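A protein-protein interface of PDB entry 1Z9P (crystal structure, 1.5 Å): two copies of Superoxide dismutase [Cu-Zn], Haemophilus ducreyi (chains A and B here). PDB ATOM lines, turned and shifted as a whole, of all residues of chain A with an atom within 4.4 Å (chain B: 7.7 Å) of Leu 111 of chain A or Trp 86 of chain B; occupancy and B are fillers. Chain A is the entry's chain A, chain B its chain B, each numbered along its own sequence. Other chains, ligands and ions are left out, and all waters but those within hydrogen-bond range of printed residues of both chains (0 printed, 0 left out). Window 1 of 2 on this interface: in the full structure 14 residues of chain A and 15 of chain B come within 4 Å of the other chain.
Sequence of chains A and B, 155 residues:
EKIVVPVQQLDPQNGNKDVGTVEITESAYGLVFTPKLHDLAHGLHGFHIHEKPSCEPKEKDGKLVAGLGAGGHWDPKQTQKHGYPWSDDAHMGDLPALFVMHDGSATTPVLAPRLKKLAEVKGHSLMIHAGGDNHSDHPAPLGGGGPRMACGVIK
The backbone NH (N) of Tyr 29 of chain A is in hydrogen-bond range of the side-chain hydroxyl (OG) of Ser 27 of chain A, 3.0 Å away.
The side-chain hydroxyl (OG) of Ser 27 of chain A lies within hydrogen-bond range of the backbone carbonyl oxygen (O) of Gly 30 of chain A (2.7 Å).
O of Tyr 84 of chain B lies within hydrogen-bond range of NH2 of Arg 114 of chain B (3.2 Å).
NE of Arg 114 of chain B sits at hydrogen-bond distance from O of Pro 85 of chain B.
The backbone carbonyl oxygen of Ser 87 of chain B lies close to the guanidinium group of Arg 114 of chain B (3.0 Å).
The guanidinium group (NH1) of Arg 114 of chain B sits at hydrogen-bond distance from the backbone carbonyl oxygen (O) of Ala 90 of chain B (3.0 Å).
Tyr 29 of chain A touches Pro 113 of chain B, and with the chains exchanged Pro 113 of chain A touches Tyr 29 of chain B.
Leu 111 of chain A touches Pro 113 of chain B, and with the chains exchanged Pro 113 of chain A touches Leu 111 of chain B.
OH of Tyr 29 of chain A lies within hydrogen-bond range of OD1 of Asp 88 of chain B (2.5 Å).
Ser 27 of chain A touches Trp 86 of chain B (OG to CB, 3.7 Å).
CD1 of Tyr 29 of chain A touches O of Trp 86 of chain B (3.4 Å).
Tyr 29 of chain A touches Pro 113 of chain B (CB to CB, 3.7 Å).
Tyr 29 of chain A touches Arg 114 of chain B.
Val 32 of chain A touches Trp 86 of chain B.
Trp 86 of chain B touches Pro 109 of chain A (CZ2 to CB, 3.8 Å).
CB of Leu 111 of chain A touches CE3 of Trp 86 of chain B, at 3.7 Å.
CD2 of Leu 111 of chain A touches CG of Pro 113 of chain B, at 3.7 Å.
Pro 113 of chain A touches Tyr 29 of chain B (CB to CB, 3.8 Å).
Pro 113 of chain A touches Leu 111 of chain B (CG to CD2, 3.6 Å).
Printed residues of chain A that touch a printed residue of chain B: Ser 27, Tyr 29, Val 32, Pro 109, Leu 111 and Pro 113.
Among the printed residues, 11 pairs touch across the chains.
Among the printed residues, no Asp or Glu carboxylate lies within 4 Å of a Lys or Arg side-chain nitrogen of the other chain.
Leu 111 of chain A touches just these residues of chain B: Trp 86 and Pro 113.
Of chain A, only Ser 27, Tyr 29, Val 32, Pro 109 and Leu 111 come within 4 Å of Trp 86 of chain B.
Of the printed residues of chain A, Arg 114 of chain B touches Tyr 29 (3.5 Å).
Of the printed residues of chain B, Val 32 of chain A touches Trp 86.
Asp 94 of chain B touches none of the printed residues of chain A.
Ala 112 of chain B touches none of the printed residues of chain A.
The nearest residue of chain B that does not touch Leu 111 of chain A is Leu 111 of chain B (4.3 Å).
The nearest residue of chain A that does not touch Trp 86 of chain B is Val 110 of chain A (4.3 Å).
The nearest printed residue of chain A that does not touch Tyr 29 of chain B is Tyr 29 of chain A (5.7 Å).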
ATOM      1  N   SER A  27      21.076  10.163  10.586  1.00  0.00           N
ATOM      2  CA  SER A  27      22.451  10.523  10.437  1.00  0.00           C
ATOM      3  C   SER A  27      23.099  10.623  11.814  1.00  0.00           C
ATOM      4  O   SER A  27      22.413  10.590  12.843  1.00  0.00           O
ATOM      5  CB  SER A  27      22.591  11.881   9.714  1.00  0.00           C
ATOM      6  OG  SER A  27      22.471  12.978  10.628  1.00  0.00           O
ATOM      7  N   TYR A  29      24.008  13.171  13.148  1.00  0.00           N
ATOM      8  CA  TYR A  29      23.662  14.495  13.639  1.00  0.00           C
ATOM      9  C   TYR A  29      22.152  14.727  13.685  1.00  0.00           C
ATOM     10  O   TYR A  29      21.686  15.863  13.931  1.00  0.00           O
ATOM     11  CB  TYR A  29      24.364  15.588  12.766  1.00  0.00           C
ATOM     12  CG  TYR A  29      25.841  15.415  12.860  1.00  0.00           C
ATOM     13  CD1 TYR A  29      26.531  14.639  11.945  1.00  0.00           C
ATOM     14  CD2 TYR A  29      26.550  15.927  13.946  1.00  0.00           C
ATOM     15  CE1 TYR A  29      27.943  14.377  12.094  1.00  0.00           C
ATOM     16  CE2 TYR A  29      27.942  15.703  14.077  1.00  0.00           C
ATOM     17  CZ  TYR A  29      28.624  14.934  13.158  1.00  0.00           C
ATOM     18  OH  TYR A  29      30.025  14.720  13.258  1.00  0.00           O
ATOM     19  N   GLY A  30      21.361  13.680  13.529  1.00  0.00           N
ATOM     20  CA  GLY A  30      19.922  13.769  13.585  1.00  0.00           C
ATOM     21  C   GLY A  30      19.237  13.241  12.351  1.00  0.00           C
ATOM     22  O   GLY A  30      19.877  12.754  11.410  1.00  0.00           O
ATOM     23  N   LEU A  31      17.911  13.362  12.330  1.00  0.00           N
ATOM     24  CA  LEU A  31      17.106  12.817  11.223  1.00  0.00           C
ATOM     25  C   LEU A  31      17.215  13.726   9.991  1.00  0.00           C
ATOM     26  O   LEU A  31      17.064  14.953  10.117  1.00  0.00           O
ATOM     27  CB  LEU A  31      15.632  12.618  11.605  1.00  0.00           C
ATOM     28  CG  LEU A  31      15.364  11.639  12.759  1.00  0.00           C
ATOM     29  CD1 LEU A  31      13.873  11.389  12.832  1.00  0.00           C
ATOM     30  CD2 LEU A  31      16.148  10.317  12.574  1.00  0.00           C
ATOM     31  N   VAL A  32      17.419  13.097   8.840  1.00  0.00           N
ATOM     32  CA  VAL A  32      17.497  13.765   7.542  1.00  0.00           C
ATOM     33  C   VAL A  32      16.193  13.498   6.812  1.00  0.00           C
ATOM     34  O   VAL A  32      15.756  12.353   6.669  1.00  0.00           O
ATOM     35  CB  VAL A  32      18.695  13.260   6.780  1.00  0.00           C
ATOM     36  CG1 VAL A  32      18.715  13.837   5.368  1.00  0.00           C
ATOM     37  CG2 VAL A  32      19.994  13.643   7.477  1.00  0.00           C
ATOM     38  N   PRO A  96      13.662  22.463   9.086  1.00  0.00           N
ATOM     39  CA  PRO A  96      14.076  23.497   8.100  1.00  0.00           C
ATOM     40  C   PRO A  96      13.045  23.570   6.974  1.00  0.00           C
ATOM     41  O   PRO A  96      12.450  22.549   6.624  1.00  0.00           O
ATOM     42  CB  PRO A  96      15.410  23.016   7.602  1.00  0.00           C
ATOM     43  CG  PRO A  96      15.951  22.136   8.694  1.00  0.00           C
ATOM     44  CD  PRO A  96      14.720  21.448   9.243  1.00  0.00           C
ATOM     45  N   PRO A 109      17.632  17.783   0.611  1.00  0.00           N
ATOM     46  CA  PRO A 109      17.503  17.222   1.973  1.00  0.00           C
ATOM     47  C   PRO A 109      17.701  18.283   3.049  1.00  0.00           C
ATOM     48  O   PRO A 109      18.465  19.249   2.831  1.00  0.00           O
ATOM     49  CB  PRO A 109      18.620  16.224   2.036  1.00  0.00           C
ATOM     50  CG  PRO A 109      19.630  16.724   1.162  1.00  0.00           C
ATOM     51  CD  PRO A 109      18.904  17.371   0.057  1.00  0.00           C
ATOM     52  N   VAL A 110      17.046  18.074   4.208  1.00  0.00           N
ATOM     53  CA  VAL A 110      17.216  18.944   5.364  1.00  0.00           C
ATOM     54  C   VAL A 110      17.339  18.162   6.634  1.00  0.00           C
ATOM     55  O   VAL A 110      16.813  17.053   6.709  1.00  0.00           O
ATOM     56  CB  VAL A 110      16.085  19.953   5.510  1.00  0.00           C
ATOM     57  CG1 VAL A 110      15.991  20.869   4.273  1.00  0.00           C
ATOM     58  CG2 VAL A 110      14.777  19.284   5.790  1.00  0.00           C
ATOM     59  N   LEU A 111      18.074  18.706   7.583  1.00  0.00           N
ATOM     60  CA  LEU A 111      18.381  18.023   8.849  1.00  0.00           C
ATOM     61  C   LEU A 111      17.557  18.598   9.986  1.00  0.00           C
ATOM     62  O   LEU A 111      17.454  19.807  10.174  1.00  0.00           O
ATOM     63  CB  LEU A 111      19.843  18.209   9.171  1.00  0.00           C
ATOM     64  CG  LEU A 111      20.347  17.640  10.507  1.00  0.00           C
ATOM     65  CD1 LEU A 111      20.401  16.140  10.467  1.00  0.00           C
ATOM     66  CD2 LEU A 111      21.685  18.240  10.876  1.00  0.00           C
ATOM     67  N   ALA A 112      17.048  17.702  10.834  1.00  0.00           N
ATOM     68  CA  ALA A 112      16.363  18.047  12.080  1.00  0.00           C
ATOM     69  C   ALA A 112      17.276  17.584  13.224  1.00  0.00           C
ATOM     70  O   ALA A 112      17.189  16.415  13.619  1.00  0.00           O
ATOM     71  CB  ALA A 112      14.996  17.362  12.127  1.00  0.00           C
ATOM     72  N   PRO A 113      18.159  18.434  13.741  1.00  0.00           N
ATOM     73  CA  PRO A 113      19.186  17.961  14.681  1.00  0.00           C
ATOM     74  C   PRO A 113      18.650  17.498  16.027  1.00  0.00           C
ATOM     75  O   PRO A 113      19.375  16.766  16.737  1.00  0.00           O
ATOM     76  CB  PRO A 113      20.045  19.192  14.897  1.00  0.00           C
ATOM     77  CG  PRO A 113      19.130  20.355  14.625  1.00  0.00           C
ATOM     78  CD  PRO A 113      18.298  19.893  13.472  1.00  0.00           C
ATOM     79  N   TYR B  29      23.446  22.672  18.727  1.00  0.00           N
ATOM     80  CA  TYR B  29      23.635  21.603  17.750  1.00  0.00           C
ATOM     81  C   TYR B  29      24.706  21.859  16.671  1.00  0.00           C
ATOM     82  O   TYR B  29      24.870  21.059  15.770  1.00  0.00           O
ATOM     83  CB  TYR B  29      22.257  21.289  17.095  1.00  0.00           C
ATOM     84  CG  TYR B  29      21.287  20.887  18.150  1.00  0.00           C
ATOM     85  CD1 TYR B  29      20.439  21.789  18.761  1.00  0.00           C
ATOM     86  CD2 TYR B  29      21.324  19.606  18.636  1.00  0.00           C
ATOM     87  CE1 TYR B  29      19.605  21.412  19.810  1.00  0.00           C
ATOM     88  CE2 TYR B  29      20.531  19.224  19.658  1.00  0.00           C
ATOM     89  CZ  TYR B  29      19.660  20.107  20.247  1.00  0.00           C
ATOM     90  OH  TYR B  29      18.866  19.724  21.301  1.00  0.00           O
ATOM     91  N   GLY B  83      30.501  16.181   0.253  1.00  0.00           N
ATOM     92  CA  GLY B  83      29.356  15.415   0.730  1.00  0.00           C
ATOM     93  C   GLY B  83      28.336  16.245   1.481  1.00  0.00           C
ATOM     94  O   GLY B  83      28.179  17.438   1.223  1.00  0.00           O
ATOM     95  N   TYR B  84      27.597  15.589   2.375  1.00  0.00           N
ATOM     96  CA  TYR B  84      26.544  16.229   3.097  1.00  0.00           C
ATOM     97  C   TYR B  84      27.027  16.962   4.312  1.00  0.00           C
ATOM     98  O   TYR B  84      28.033  16.611   4.908  1.00  0.00           O
ATOM     99  CB  TYR B  84      25.546  15.160   3.572  1.00  0.00           C
ATOM    100  CG  TYR B  84      24.810  14.465   2.463  1.00  0.00           C
ATOM    101  CD1 TYR B  84      25.204  13.227   2.028  1.00  0.00           C
ATOM    102  CD2 TYR B  84      23.700  15.033   1.868  1.00  0.00           C
ATOM    103  CE1 TYR B  84      24.490  12.580   1.040  1.00  0.00           C
ATOM    104  CE2 TYR B  84      23.020  14.416   0.817  1.00  0.00           C
ATOM    105  CZ  TYR B  84      23.431  13.172   0.431  1.00  0.00           C
ATOM    106  OH  TYR B  84      22.718  12.517  -0.579  1.00  0.00           O
ATOM    107  N   PRO B  85      26.271  17.961   4.782  1.00  0.00           N
ATOM    108  CA  PRO B  85      26.698  18.653   6.004  1.00  0.00           C
ATOM    109  C   PRO B  85      26.706  17.733   7.235  1.00  0.00           C
ATOM    110  O   PRO B  85      27.372  18.079   8.232  1.00  0.00           O
ATOM    111  CB  PRO B  85      25.676  19.807   6.118  1.00  0.00           C
ATOM    112  CG  PRO B  85      25.232  19.985   4.702  1.00  0.00           C
ATOM    113  CD  PRO B  85      25.101  18.607   4.147  1.00  0.00           C
ATOM    114  N   TRP B  86      25.962  16.632   7.173  1.00  0.00           N
ATOM    115  CA  TRP B  86      25.780  15.715   8.288  1.00  0.00           C
ATOM    116  C   TRP B  86      26.580  14.411   8.090  1.00  0.00           C
ATOM    117  O   TRP B  86      26.285  13.417   8.813  1.00  0.00           O
ATOM    118  CB  TRP B  86      24.292  15.409   8.522  1.00  0.00           C
ATOM    119  CG  TRP B  86      23.555  15.198   7.239  1.00  0.00           C
ATOM    120  CD1 TRP B  86      23.453  14.050   6.519  1.00  0.00           C
ATOM    121  CD2 TRP B  86      22.817  16.197   6.500  1.00  0.00           C
ATOM    122  NE1 TRP B  86      22.733  14.265   5.372  1.00  0.00           N
ATOM    123  CE2 TRP B  86      22.321  15.573   5.341  1.00  0.00           C
ATOM    124  CE3 TRP B  86      22.505  17.556   6.720  1.00  0.00           C
ATOM    125  CZ2 TRP B  86      21.532  16.254   4.399  1.00  0.00           C
ATOM    126  CZ3 TRP B  86      21.758  18.221   5.775  1.00  0.00           C
ATOM    127  CH2 TRP B  86      21.275  17.554   4.648  1.00  0.00           C
ATOM    128  N   SER B  87      27.533  14.416   7.170  1.00  0.00           N
ATOM    129  CA  SER B  87      28.354  13.225   6.916  1.00  0.00           C
ATOM    130  C   SER B  87      29.772  13.467   7.370  1.00  0.00           C
ATOM    131  O   SER B  87      30.445  14.407   6.973  1.00  0.00           O
ATOM    132  CB  SER B  87      28.303  12.814   5.464  1.00  0.00           C
ATOM    133  OG  SER B  87      29.161  11.711   5.261  1.00  0.00           O
ATOM    134  N   ASP B  88      30.272  12.560   8.206  1.00  0.00           N
ATOM    135  CA  ASP B  88      31.628  12.672   8.668  1.00  0.00           C
ATOM    136  C   ASP B  88      32.660  12.316   7.602  1.00  0.00           C
ATOM    137  O   ASP B  88      33.833  12.572   7.820  1.00  0.00           O
ATOM    138  CB  ASP B  88      31.814  11.810   9.930  1.00  0.00           C
ATOM    139  CG  ASP B  88      31.110  12.406  11.132  1.00  0.00           C
ATOM    140  OD1 ASP B  88      31.288  13.614  11.381  1.00  0.00           O
ATOM    141  OD2 ASP B  88      30.338  11.731  11.866  1.00  0.00           O
ATOM    142  N   ASP B  89      32.260  11.778   6.452  1.00  0.00           N
ATOM    143  CA  ASP B  89      33.237  11.442   5.394  1.00  0.00           C
ATOM    144  C   ASP B  89      33.414  12.543   4.345  1.00  0.00           C
ATOM    145  O   ASP B  89      34.085  12.358   3.328  1.00  0.00           O
ATOM    146  CB  ASP B  89      32.891  10.095   4.749  1.00  0.00           C
ATOM    147  CG  ASP B  89      31.652  10.132   3.929  1.00  0.00           C
ATOM    148  OD1 ASP B  89      30.976  11.186   3.898  1.00  0.00           O
ATOM    149  OD2 ASP B  89      31.259   9.128   3.281  1.00  0.00           O
ATOM    150  N   ALA B  90      32.894  13.717   4.658  1.00  0.00           N
ATOM    151  CA  ALA B  90      32.856  14.821   3.701  1.00  0.00           C
ATOM    152  C   ALA B  90      33.721  15.979   4.173  1.00  0.00           C
ATOM    153  O   ALA B  90      34.038  16.101   5.346  1.00  0.00           O
ATOM    154  CB  ALA B  90      31.438  15.283   3.544  1.00  0.00           C
ATOM    155  N   ASP B  94      31.592  21.702   4.202  1.00  0.00           N
ATOM    156  CA  ASP B  94      30.346  21.502   3.425  1.00  0.00           C
ATOM    157  C   ASP B  94      29.148  21.915   4.213  1.00  0.00           C
ATOM    158  O   ASP B  94      28.806  21.283   5.207  1.00  0.00           O
ATOM    159  CB  ASP B  94      30.220  20.058   2.936  1.00  0.00           C
ATOM    160  CG  ASP B  94      31.290  19.698   1.911  1.00  0.00           C
ATOM    161  OD1 ASP B  94      31.909  20.652   1.323  1.00  0.00           O
ATOM    162  OD2 ASP B  94      31.569  18.507   1.560  1.00  0.00           O
ATOM    163  N   LEU B  95      28.498  23.014   3.783  1.00  0.00           N
ATOM    164  CA  LEU B  95      27.348  23.545   4.472  1.00  0.00           C
ATOM    165  C   LEU B  95      26.075  23.284   3.681  1.00  0.00           C
ATOM    166  O   LEU B  95      26.117  22.933   2.489  1.00  0.00           O
ATOM    167  CB  LEU B  95      27.441  25.070   4.673  1.00  0.00           C
ATOM    168  CG  LEU B  95      28.812  25.561   5.135  1.00  0.00           C
ATOM    169  CD1 LEU B  95      28.824  27.109   5.139  1.00  0.00           C
ATOM    170  CD2 LEU B  95      29.185  25.079   6.539  1.00  0.00           C
ATOM    171  N   PRO B  96      24.903  23.398   4.323  1.00  0.00           N
ATOM    172  CA  PRO B  96      23.649  23.311   3.582  1.00  0.00           C
ATOM    173  C   PRO B  96      23.587  24.417   2.523  1.00  0.00           C
ATOM    174  O   PRO B  96      24.137  25.504   2.730  1.00  0.00           O
ATOM    175  CB  PRO B  96      22.562  23.509   4.643  1.00  0.00           C
ATOM    176  CG  PRO B  96      23.230  23.129   5.897  1.00  0.00           C
ATOM    177  CD  PRO B  96      24.673  23.559   5.771  1.00  0.00           C
ATOM    178  N   ALA B  97      22.928  24.154   1.411  1.00  0.00           N
ATOM    179  CA  ALA B  97      22.836  25.175   0.357  1.00  0.00           C
ATOM    180  C   ALA B  97      22.008  26.379   0.756  1.00  0.00           C
ATOM    181  O   ALA B  97      21.127  26.283   1.599  1.00  0.00           O
ATOM    182  CB  ALA B  97      22.244  24.525  -0.904  1.00  0.00           C
ATOM    183  N   LEU B 111      22.108  25.304   9.388  1.00  0.00           N
ATOM    184  CA  LEU B 111      22.921  24.712  10.452  1.00  0.00           C
ATOM    185  C   LEU B 111      24.027  23.815   9.874  1.00  0.00           C
ATOM    186  O   LEU B 111      23.752  22.995   8.986  1.00  0.00           O
ATOM    187  CB  LEU B 111      22.013  23.884  11.359  1.00  0.00           C
ATOM    188  CG  LEU B 111      22.790  23.026  12.373  1.00  0.00           C
ATOM    189  CD1 LEU B 111      23.311  23.944  13.481  1.00  0.00           C
ATOM    190  CD2 LEU B 111      21.910  21.979  12.981  1.00  0.00           C
ATOM    191  N   ALA B 112      25.254  23.950  10.381  1.00  0.00           N
ATOM    192  CA  ALA B 112      26.377  23.064  10.070  1.00  0.00           C
ATOM    193  C   ALA B 112      26.689  22.258  11.339  1.00  0.00           C
ATOM    194  O   ALA B 112      27.471  22.708  12.167  1.00  0.00           O
ATOM    195  CB  ALA B 112      27.585  23.832   9.642  1.00  0.00           C
ATOM    196  N   PRO B 113      26.080  21.081  11.472  1.00  0.00           N
ATOM    197  CA  PRO B 113      26.155  20.339  12.782  1.00  0.00           C
ATOM    198  C   PRO B 113      27.541  19.799  13.106  1.00  0.00           C
ATOM    199  O   PRO B 113      27.819  19.568  14.294  1.00  0.00           O
ATOM    200  CB  PRO B 113      25.195  19.175  12.569  1.00  0.00           C
ATOM    201  CG  PRO B 113      25.291  18.903  11.072  1.00  0.00           C
ATOM    202  CD  PRO B 113      25.283  20.334  10.492  1.00  0.00           C
ATOM    203  N   ARG B 114      28.404  19.646  12.115  1.00  0.00           N
ATOM    204  CA  ARG B 114      29.762  19.140  12.322  1.00  0.00           C
ATOM    205  C   ARG B 114      30.660  20.228  12.854  1.00  0.00           C
ATOM    206  O   ARG B 114      31.725  19.901  13.380  1.00  0.00           O
ATOM    207  CB  ARG B 114      30.357  18.488  11.105  1.00  0.00           C
ATOM    208  CG  ARG B 114      29.591  17.240  10.682  1.00  0.00           C
ATOM    209  CD  ARG B 114      30.263  16.440   9.636  1.00  0.00           C
ATOM    210  NE  ARG B 114      30.091  17.032   8.314  1.00  0.00           N
ATOM    211  CZ  ARG B 114      31.057  17.256   7.397  1.00  0.00           C
ATOM    212  NH1 ARG B 114      32.340  16.954   7.630  1.00  0.00           N
ATOM    213  NH2 ARG B 114      30.715  17.762   6.218  1.00  0.00           N
ATOM    214  N   HIS B 135      25.476  17.644  -2.839  1.00  0.00           N
ATOM    215  CA  HIS B 135      26.250  17.004  -1.814  1.00  0.00           C
ATOM    216  C   HIS B 135      26.924  15.736  -2.265  1.00  0.00           C
ATOM    217  O   HIS B 135      27.084  14.779  -1.512  1.00  0.00           O
ATOM    218  CB  HIS B 135      25.396  16.775  -0.559  1.00  0.00           C
ATOM    219  CG  HIS B 135      24.862  18.062   0.028  1.00  0.00           C
ATOM    220  ND1 HIS B 135      25.692  19.025   0.556  1.00  0.00           N
ATOM    221  CD2 HIS B 135      23.610  18.566   0.094  1.00  0.00           C
ATOM    222  CE1 HIS B 135      24.972  20.074   0.921  1.00  0.00           C
ATOM    223  NE2 HIS B 135      23.700  19.820   0.675  1.00  0.00           N
